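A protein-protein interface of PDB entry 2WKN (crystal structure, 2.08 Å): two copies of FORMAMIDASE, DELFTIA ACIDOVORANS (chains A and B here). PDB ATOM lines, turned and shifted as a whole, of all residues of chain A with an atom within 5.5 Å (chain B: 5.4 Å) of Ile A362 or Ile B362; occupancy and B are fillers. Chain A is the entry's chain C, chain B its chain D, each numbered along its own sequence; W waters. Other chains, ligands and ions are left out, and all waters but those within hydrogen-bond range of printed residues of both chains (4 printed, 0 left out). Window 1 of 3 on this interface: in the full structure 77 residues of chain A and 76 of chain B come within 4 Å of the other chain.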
ATOM      1  N   ASP A 257      -8.277   9.419  24.066  1.00  0.00           N
ATOM      2  CA  ASP A 257      -8.263   8.433  25.133  1.00  0.00           C
ATOM      3  C   ASP A 257      -6.803   8.296  25.652  1.00  0.00           C
ATOM      4  O   ASP A 257      -5.845   8.240  24.861  1.00  0.00           O
ATOM      5  CB  ASP A 257      -8.790   7.073  24.639  1.00  0.00           C
ATOM      6  CG  ASP A 257     -10.267   6.813  25.009  1.00  0.00           C
ATOM      7  OD1 ASP A 257     -10.922   7.582  25.774  1.00  0.00           O
ATOM      8  OD2 ASP A 257     -10.810   5.817  24.495  1.00  0.00           O
ATOM      9  N   GLY A 258      -6.650   8.287  26.970  1.00  0.00           N
ATOM     10  CA  GLY A 258      -5.314   8.177  27.573  1.00  0.00           C
ATOM     11  C   GLY A 258      -4.746   9.531  27.963  1.00  0.00           C
ATOM     12  O   GLY A 258      -3.928   9.606  28.874  1.00  0.00           O
ATOM     13  N   VAL A 324      -1.002  -3.730  29.484  1.00  0.00           N
ATOM     14  CA  VAL A 324      -1.805  -2.893  28.561  1.00  0.00           C
ATOM     15  C   VAL A 324      -1.104  -1.562  28.299  1.00  0.00           C
ATOM     16  O   VAL A 324      -1.124  -1.031  27.169  1.00  0.00           O
ATOM     17  CB  VAL A 324      -3.211  -2.641  29.094  1.00  0.00           C
ATOM     18  CG1 VAL A 324      -4.035  -1.833  28.108  1.00  0.00           C
ATOM     19  CG2 VAL A 324      -3.923  -3.971  29.450  1.00  0.00           C
ATOM     20  N   TYR A 328      -0.448  -0.180  24.642  1.00  0.00           N
ATOM     21  CA  TYR A 328      -1.004   1.103  24.160  1.00  0.00           C
ATOM     22  C   TYR A 328       0.082   1.998  23.580  1.00  0.00           C
ATOM     23  O   TYR A 328      -0.114   2.596  22.545  1.00  0.00           O
ATOM     24  CB  TYR A 328      -1.799   1.835  25.241  1.00  0.00           C
ATOM     25  CG  TYR A 328      -2.733   2.931  24.724  1.00  0.00           C
ATOM     26  CD1 TYR A 328      -3.610   2.703  23.649  1.00  0.00           C
ATOM     27  CD2 TYR A 328      -2.768   4.178  25.337  1.00  0.00           C
ATOM     28  CE1 TYR A 328      -4.462   3.693  23.181  1.00  0.00           C
ATOM     29  CE2 TYR A 328      -3.623   5.185  24.876  1.00  0.00           C
ATOM     30  CZ  TYR A 328      -4.465   4.924  23.791  1.00  0.00           C
ATOM     31  OH  TYR A 328      -5.305   5.894  23.334  1.00  0.00           O
ATOM     32  N   GLY A 360      -9.032   4.514  22.581  1.00  0.00           N
ATOM     33  CA  GLY A 360      -8.014   3.564  23.011  1.00  0.00           C
ATOM     34  C   GLY A 360      -8.757   2.446  23.685  1.00  0.00           C
ATOM     35  O   GLY A 360      -9.385   2.651  24.745  1.00  0.00           O
ATOM     36  N   HIS A 361      -8.696   1.267  23.075  1.00  0.00           N
ATOM     37  CA  HIS A 361      -9.367   0.110  23.616  1.00  0.00           C
ATOM     38  C   HIS A 361      -8.429  -0.916  24.218  1.00  0.00           C
ATOM     39  O   HIS A 361      -7.344  -1.193  23.701  1.00  0.00           O
ATOM     40  CB  HIS A 361     -10.200  -0.559  22.567  1.00  0.00           C
ATOM     41  CG  HIS A 361     -11.437   0.196  22.200  1.00  0.00           C
ATOM     42  ND1 HIS A 361     -12.690  -0.231  22.565  1.00  0.00           N
ATOM     43  CD2 HIS A 361     -11.623   1.321  21.470  1.00  0.00           C
ATOM     44  CE1 HIS A 361     -13.599   0.603  22.088  1.00  0.00           C
ATOM     45  NE2 HIS A 361     -12.979   1.561  21.429  1.00  0.00           N
ATOM     46  N   ILE A 362      -8.896  -1.478  25.316  1.00  0.00           N
ATOM     47  CA  ILE A 362      -8.312  -2.654  25.901  1.00  0.00           C
ATOM     48  C   ILE A 362      -8.939  -3.846  25.182  1.00  0.00           C
ATOM     49  O   ILE A 362      -9.874  -4.484  25.674  1.00  0.00           O
ATOM     50  CB  ILE A 362      -8.603  -2.701  27.450  1.00  0.00           C
ATOM     51  CG1 ILE A 362      -8.219  -1.364  28.102  1.00  0.00           C
ATOM     52  CG2 ILE A 362      -7.850  -3.871  28.081  1.00  0.00           C
ATOM     53  CD1 ILE A 362      -8.689  -1.170  29.560  1.00  0.00           C
ATOM     54  N   SER A 363      -8.444  -4.139  23.991  1.00  0.00           N
ATOM     55  CA  SER A 363      -9.096  -5.132  23.121  1.00  0.00           C
ATOM     56  C   SER A 363      -8.953  -6.551  23.671  1.00  0.00           C
ATOM     57  O   SER A 363      -9.927  -7.293  23.669  1.00  0.00           O
ATOM     58  CB  SER A 363      -8.594  -5.050  21.685  1.00  0.00           C
ATOM     59  OG  SER A 363      -8.863  -3.760  21.154  1.00  0.00           O
ATOM     60  N   GLY A 364      -7.760  -6.883  24.192  1.00  0.00           N
ATOM     61  CA  GLY A 364      -7.507  -8.173  24.819  1.00  0.00           C
ATOM     62  C   GLY A 364      -6.572  -8.094  26.011  1.00  0.00           C
ATOM     63  O   GLY A 364      -5.545  -7.418  25.973  1.00  0.00           O
ATOM     64  N   VAL A 365      -6.914  -8.804  27.076  1.00  0.00           N
ATOM     65  CA  VAL A 365      -6.101  -8.749  28.281  1.00  0.00           C
ATOM     66  C   VAL A 365      -5.925 -10.144  28.920  1.00  0.00           C
ATOM     67  O   VAL A 365      -5.835 -10.303  30.145  1.00  0.00           O
ATOM     68  CB  VAL A 365      -6.636  -7.653  29.227  1.00  0.00           C
ATOM     69  CG1 VAL A 365      -7.910  -8.102  29.928  1.00  0.00           C
ATOM     70  CG2 VAL A 365      -5.562  -7.225  30.219  1.00  0.00           C
ATOM     71  N   CYS A 372      -3.518  -6.943  24.161  1.00  0.00           N
ATOM     72  CA  CYS A 372      -3.683  -6.255  22.873  1.00  0.00           C
ATOM     73  C   CYS A 372      -4.454  -4.962  23.088  1.00  0.00           C
ATOM     74  O   CYS A 372      -5.590  -4.982  23.572  1.00  0.00           O
ATOM     75  CB  CYS A 372      -4.449  -7.137  21.864  1.00  0.00           C
ATOM     76  SG  CYS A 372      -4.602  -6.433  20.212  1.00  0.00           S
ATOM     77  N   ALA A 373      -3.853  -3.844  22.673  1.00  0.00           N
ATOM     78  CA  ALA A 373      -4.478  -2.539  22.795  1.00  0.00           C
ATOM     79  C   ALA A 373      -4.587  -1.916  21.424  1.00  0.00           C
ATOM     80  O   ALA A 373      -3.657  -2.063  20.612  1.00  0.00           O
ATOM     81  CB  ALA A 373      -3.665  -1.659  23.727  1.00  0.00           C
ATOM     82  N   THR A 374      -5.706  -1.227  21.168  1.00  0.00           N
ATOM     83  CA  THR A 374      -5.923  -0.520  19.884  1.00  0.00           C
ATOM     84  C   THR A 374      -6.102   0.997  20.059  1.00  0.00           C
ATOM     85  O   THR A 374      -6.624   1.481  21.081  1.00  0.00           O
ATOM     86  CB  THR A 374      -7.145  -1.089  19.147  1.00  0.00           C
ATOM     87  OG1 THR A 374      -8.207  -1.320  20.106  1.00  0.00           O
ATOM     88  CG2 THR A 374      -6.787  -2.407  18.506  1.00  0.00           C
ATOM     89  N   ASP B 257     -14.716  -6.314  25.187  1.00  0.00           N
ATOM     90  CA  ASP B 257     -13.357  -5.813  25.176  1.00  0.00           C
ATOM     91  C   ASP B 257     -12.570  -6.488  26.304  1.00  0.00           C
ATOM     92  O   ASP B 257     -13.050  -6.568  27.450  1.00  0.00           O
ATOM     93  CB  ASP B 257     -13.339  -4.294  25.344  1.00  0.00           C
ATOM     94  CG  ASP B 257     -13.284  -3.537  23.996  1.00  0.00           C
ATOM     95  OD1 ASP B 257     -12.987  -4.154  22.946  1.00  0.00           O
ATOM     96  OD2 ASP B 257     -13.541  -2.316  24.004  1.00  0.00           O
ATOM     97  N   GLY B 258     -11.379  -6.978  25.973  1.00  0.00           N
ATOM     98  CA  GLY B 258     -10.504  -7.626  26.964  1.00  0.00           C
ATOM     99  C   GLY B 258     -10.639  -9.138  26.910  1.00  0.00           C
ATOM    100  O   GLY B 258      -9.738  -9.854  27.314  1.00  0.00           O
ATOM    101  N   VAL B 324      -2.818   0.144  33.796  1.00  0.00           N
ATOM    102  CA  VAL B 324      -4.139   0.022  33.176  1.00  0.00           C
ATOM    103  C   VAL B 324      -4.762  -1.342  33.448  1.00  0.00           C
ATOM    104  O   VAL B 324      -5.986  -1.458  33.552  1.00  0.00           O
ATOM    105  CB  VAL B 324      -4.082   0.228  31.662  1.00  0.00           C
ATOM    106  CG1 VAL B 324      -5.503   0.140  31.060  1.00  0.00           C
ATOM    107  CG2 VAL B 324      -3.451   1.581  31.322  1.00  0.00           C
ATOM    108  N   TYR B 328      -8.467  -1.755  34.944  1.00  0.00           N
ATOM    109  CA  TYR B 328      -9.570  -2.412  34.228  1.00  0.00           C
ATOM    110  C   TYR B 328     -10.188  -3.496  35.077  1.00  0.00           C
ATOM    111  O   TYR B 328     -11.393  -3.688  35.006  1.00  0.00           O
ATOM    112  CB  TYR B 328      -9.129  -2.968  32.882  1.00  0.00           C
ATOM    113  CG  TYR B 328     -10.254  -3.380  31.938  1.00  0.00           C
ATOM    114  CD1 TYR B 328     -11.266  -2.475  31.580  1.00  0.00           C
ATOM    115  CD2 TYR B 328     -10.264  -4.643  31.341  1.00  0.00           C
ATOM    116  CE1 TYR B 328     -12.260  -2.831  30.707  1.00  0.00           C
ATOM    117  CE2 TYR B 328     -11.263  -5.010  30.440  1.00  0.00           C
ATOM    118  CZ  TYR B 328     -12.259  -4.089  30.133  1.00  0.00           C
ATOM    119  OH  TYR B 328     -13.252  -4.422  29.251  1.00  0.00           O
ATOM    120  N   GLY B 360     -14.138  -1.468  26.734  1.00  0.00           N
ATOM    121  CA  GLY B 360     -13.113  -1.222  27.754  1.00  0.00           C
ATOM    122  C   GLY B 360     -12.214  -0.120  27.211  1.00  0.00           C
ATOM    123  O   GLY B 360     -11.602  -0.291  26.153  1.00  0.00           O
ATOM    124  N   HIS B 361     -12.169   1.023  27.906  1.00  0.00           N
ATOM    125  CA  HIS B 361     -11.399   2.166  27.413  1.00  0.00           C
ATOM    126  C   HIS B 361     -10.239   2.475  28.348  1.00  0.00           C
ATOM    127  O   HIS B 361     -10.364   2.372  29.601  1.00  0.00           O
ATOM    128  CB  HIS B 361     -12.267   3.401  27.284  1.00  0.00           C
ATOM    129  CG  HIS B 361     -13.143   3.412  26.069  1.00  0.00           C
ATOM    130  ND1 HIS B 361     -12.923   4.256  25.004  1.00  0.00           N
ATOM    131  CD2 HIS B 361     -14.252   2.702  25.760  1.00  0.00           C
ATOM    132  CE1 HIS B 361     -13.862   4.070  24.087  1.00  0.00           C
ATOM    133  NE2 HIS B 361     -14.673   3.121  24.519  1.00  0.00           N
ATOM    134  N   ILE B 362      -9.124   2.831  27.718  1.00  0.00           N
ATOM    135  CA  ILE B 362      -7.952   3.356  28.377  1.00  0.00           C
ATOM    136  C   ILE B 362      -8.147   4.857  28.439  1.00  0.00           C
ATOM    137  O   ILE B 362      -7.602   5.609  27.604  1.00  0.00           O
ATOM    138  CB  ILE B 362      -6.659   3.035  27.568  1.00  0.00           C
ATOM    139  CG1 ILE B 362      -6.585   1.527  27.248  1.00  0.00           C
ATOM    140  CG2 ILE B 362      -5.442   3.509  28.331  1.00  0.00           C
ATOM    141  CD1 ILE B 362      -5.511   1.123  26.216  1.00  0.00           C
ATOM    142  N   SER B 363      -8.911   5.293  29.432  1.00  0.00           N
ATOM    143  CA  SER B 363      -9.469   6.650  29.462  1.00  0.00           C
ATOM    144  C   SER B 363      -8.383   7.635  29.802  1.00  0.00           C
ATOM    145  O   SER B 363      -8.259   8.672  29.149  1.00  0.00           O
ATOM    146  CB  SER B 363     -10.665   6.734  30.443  1.00  0.00           C
ATOM    147  OG  SER B 363     -11.755   5.940  29.956  1.00  0.00           O
ATOM    148  N   GLY B 364      -7.538   7.263  30.772  1.00  0.00           N
ATOM    149  CA  GLY B 364      -6.396   8.079  31.168  1.00  0.00           C
ATOM    150  C   GLY B 364      -5.178   7.247  31.554  1.00  0.00           C
ATOM    151  O   GLY B 364      -5.275   6.277  32.316  1.00  0.00           O
ATOM    152  N   VAL B 365      -4.019   7.632  31.044  1.00  0.00           N
ATOM    153  CA  VAL B 365      -2.825   6.858  31.309  1.00  0.00           C
ATOM    154  C   VAL B 365      -1.613   7.774  31.679  1.00  0.00           C
ATOM    155  O   VAL B 365      -0.460   7.460  31.386  1.00  0.00           O
ATOM    156  CB  VAL B 365      -2.562   5.890  30.126  1.00  0.00           C
ATOM    157  CG1 VAL B 365      -2.012   6.641  28.907  1.00  0.00           C
ATOM    158  CG2 VAL B 365      -1.618   4.764  30.542  1.00  0.00           C
ATOM    159  N   CYS B 372      -6.682   5.519  34.491  1.00  0.00           N
ATOM    160  CA  CYS B 372      -8.128   5.404  34.564  1.00  0.00           C
ATOM    161  C   CYS B 372      -8.679   4.556  33.421  1.00  0.00           C
ATOM    162  O   CYS B 372      -8.549   4.911  32.239  1.00  0.00           O
ATOM    163  CB  CYS B 372      -8.795   6.786  34.526  1.00  0.00           C
ATOM    164  SG  CYS B 372     -10.581   6.723  34.889  1.00  0.00           S
ATOM    165  N   ALA B 373      -9.335   3.468  33.785  1.00  0.00           N
ATOM    166  CA  ALA B 373      -9.952   2.582  32.815  1.00  0.00           C
ATOM    167  C   ALA B 373     -11.453   2.532  33.001  1.00  0.00           C
ATOM    168  O   ALA B 373     -11.958   2.502  34.169  1.00  0.00           O
ATOM    169  CB  ALA B 373      -9.352   1.177  32.901  1.00  0.00           C
ATOM    170  N   THR B 374     -12.172   2.491  31.879  1.00  0.00           N
ATOM    171  CA  THR B 374     -13.656   2.397  31.948  1.00  0.00           C
ATOM    172  C   THR B 374     -14.226   1.145  31.267  1.00  0.00           C
ATOM    173  O   THR B 374     -13.690   0.670  30.260  1.00  0.00           O
ATOM    174  CB  THR B 374     -14.340   3.626  31.365  1.00  0.00           C
ATOM    175  OG1 THR B 374     -13.694   3.991  30.140  1.00  0.00           O
ATOM    176  CG2 THR B 374     -14.229   4.788  32.294  1.00  0.00           C
HETATM  177  O   HOH W   1     -11.687  -3.407  20.752  1.00  0.00           O
HETATM  178  O   HOH W   2     -10.665   9.811  27.481  1.00  0.00           O
HETATM  179  O   HOH W   3     -11.999  -6.357  21.784  1.00  0.00           O
HETATM  180  O   HOH W   4     -12.739   6.957  27.769  1.00  0.00           O
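The backbone NH (N) of His B361 sits at hydrogen-bond distance from the backbone carbonyl oxygen (O) of Thr B374 (2.8 Å). The side-chain carboxylate of Asp A257 sits at hydrogen-bond distance from the backbone NH of Gly A360. The side-chain hydroxyl (OH) of Tyr A328 sits at hydrogen-bond distance from the backbone carbonyl oxygen (O) of Asp A257, at 2.9 Å. The backbone carbonyl oxygen of Asp B257 sits at hydrogen-bond distance from the side-chain hydroxyl of Tyr B328 (2.8 Å). The backbone carbonyl oxygen (O) of Cys A372 lies within hydrogen-bond range of the backbone NH (N) of Ser A363, at 3.0 Å. The side-chain hydroxyl (OG) of Ser B363 lies within hydrogen-bond range of the side-chain hydroxyl (OG1) of Thr B374.
Water W4 lies within hydrogen-bond range of OG of Ser B363 and OD1 of Asp A257. Water W1 bridges the side-chain carboxylate of Asp B257 and the side-chain hydroxyl of Ser A363. Water W3 bridges the side-chain carboxylate (OD1) of Asp B257 and the backbone carbonyl oxygen (O) of Ser A363. Water W2 bridges the side-chain carboxylate (OD1) of Asp A257 (2.8 Å) and the backbone carbonyl oxygen (O) of Ser B363 (3.1 Å).
Asp A257 touches Ser B363 (C to O, 3.8 Å). CG1 of Val B324 touches CG1 of Val A324 (3.8 Å). CD1 of Tyr A328 touches CD1 of Ile B362, at 3.6 Å. Gly A360 touches Gly B360 (O to O, 3.9 Å). CA of His A361 touches O of Gly B360, at 3.4 Å. NE2 of His B361 touches CE1 of His A361 (3.7 Å). O of His A361 touches CD1 of Ile B362 (3.9 Å). O of Ile A362 touches C of Asp B257, at 3.4 Å. Val B324 touches Ile A362 (CG1 to CD1, 3.8 Å). CD1 of Ile A362 touches O of His B361, at 3.9 Å.
Of the printed residues of chain B, Val A365 touches Gly B258. Cys A372 touches none of the printed residues of chain B. Thr A374 touches none of the printed residues of chain B. Of the printed residues of chain A, Asp B257 touches His A361 (2.7 Å), Ile A362 (3.4 Å) and Ser A363 (3.8 Å). Of the printed residues of chain A, Gly B360 touches Gly A360, His A361 and Ile A362. Printed residues of chain A within 4 Å of His B361: Asp A257 (2.7 Å), Gly A360 (3.4 Å), His A361 (3.7 Å) and Ile A362 (3.9 Å). Of chain A, only Asp A257, Gly A258, Val A324, Tyr A328, Gly A360, His A361 and Ile A362 come within 4 Å of Ile B362. The nearest residue of chain A that does not touch Ile B362 is Ala A373 (4.2 Å).
Hydrophobic or aromatic side chains of chain B that line the printed part of chain A: Val B324, Tyr B328, His B361, Ile B362 and Val B365. Along chain B the printed residues that touch a printed residue of chain A span positions 257 to 365. Printed residues of chain A that touch a printed residue of chain B: Asp A257, Gly A258, Val A324, Tyr A328, Gly A360, His A361, Ile A362, Ser A363, Gly A364 and Val A365. Hydrophobic or aromatic side chains of chain A that line the printed part of chain B: Val A324, Tyr A328, His A361, Ile A362 and Val A365. Among the printed residues, no Asp or Glu carboxylate lies within 4 Å of a Lys or Arg side-chain nitrogen of the other chain.
Tyr A328 touches Ile B362, and with the chains exchanged Ile A362 touches Tyr B328. Gly A360 touches His B361, and with the chains exchanged His A361 touches Gly B360. Gly A360 touches Ile B362, and with the chains exchanged Ile A362 touches Gly B360. His A361 touches Ile B362, and with the chains exchanged Ile A362 touches His B361. Of the 28 pairs that touch across the chains among the printed residues, 28 have their exchanged pair printed and touching as well.
The side-chain carboxylate of Asp A257 lies within hydrogen-bond range of a ring nitrogen (ND1) of His B361, 2.7 Å away. N of Val A365 lies within hydrogen-bond range of O of Gly B258 (3.0 Å). The backbone carbonyl oxygen (O) of Ser A363 sits at hydrogen-bond distance from the backbone NH (N) of Gly B258, at 2.7 Å. N of Val B365 lies within hydrogen-bond range of O of Gly A258, 2.9 Å away. N of Gly A258 lies within hydrogen-bond range of O of Ser B363, at 2.7 Å. O of Ile A362 is in hydrogen-bond range of N of Gly B258, 2.9 Å away. A ring nitrogen (ND1) of His A361 sits at hydrogen-bond distance from the side-chain carboxylate (OD2) of Asp B257, 2.7 Å away. The backbone NH (N) of Ile A362 sits at hydrogen-bond distance from the backbone carbonyl oxygen (O) of Gly B360. The backbone carbonyl oxygen of Ile B362 sits at hydrogen-bond distance from the backbone NH of Gly A258 (2.9 Å). The backbone carbonyl oxygen (O) of Gly A360 is in hydrogen-bond range of the backbone NH (N) of Ile B362, 3.0 Å away.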
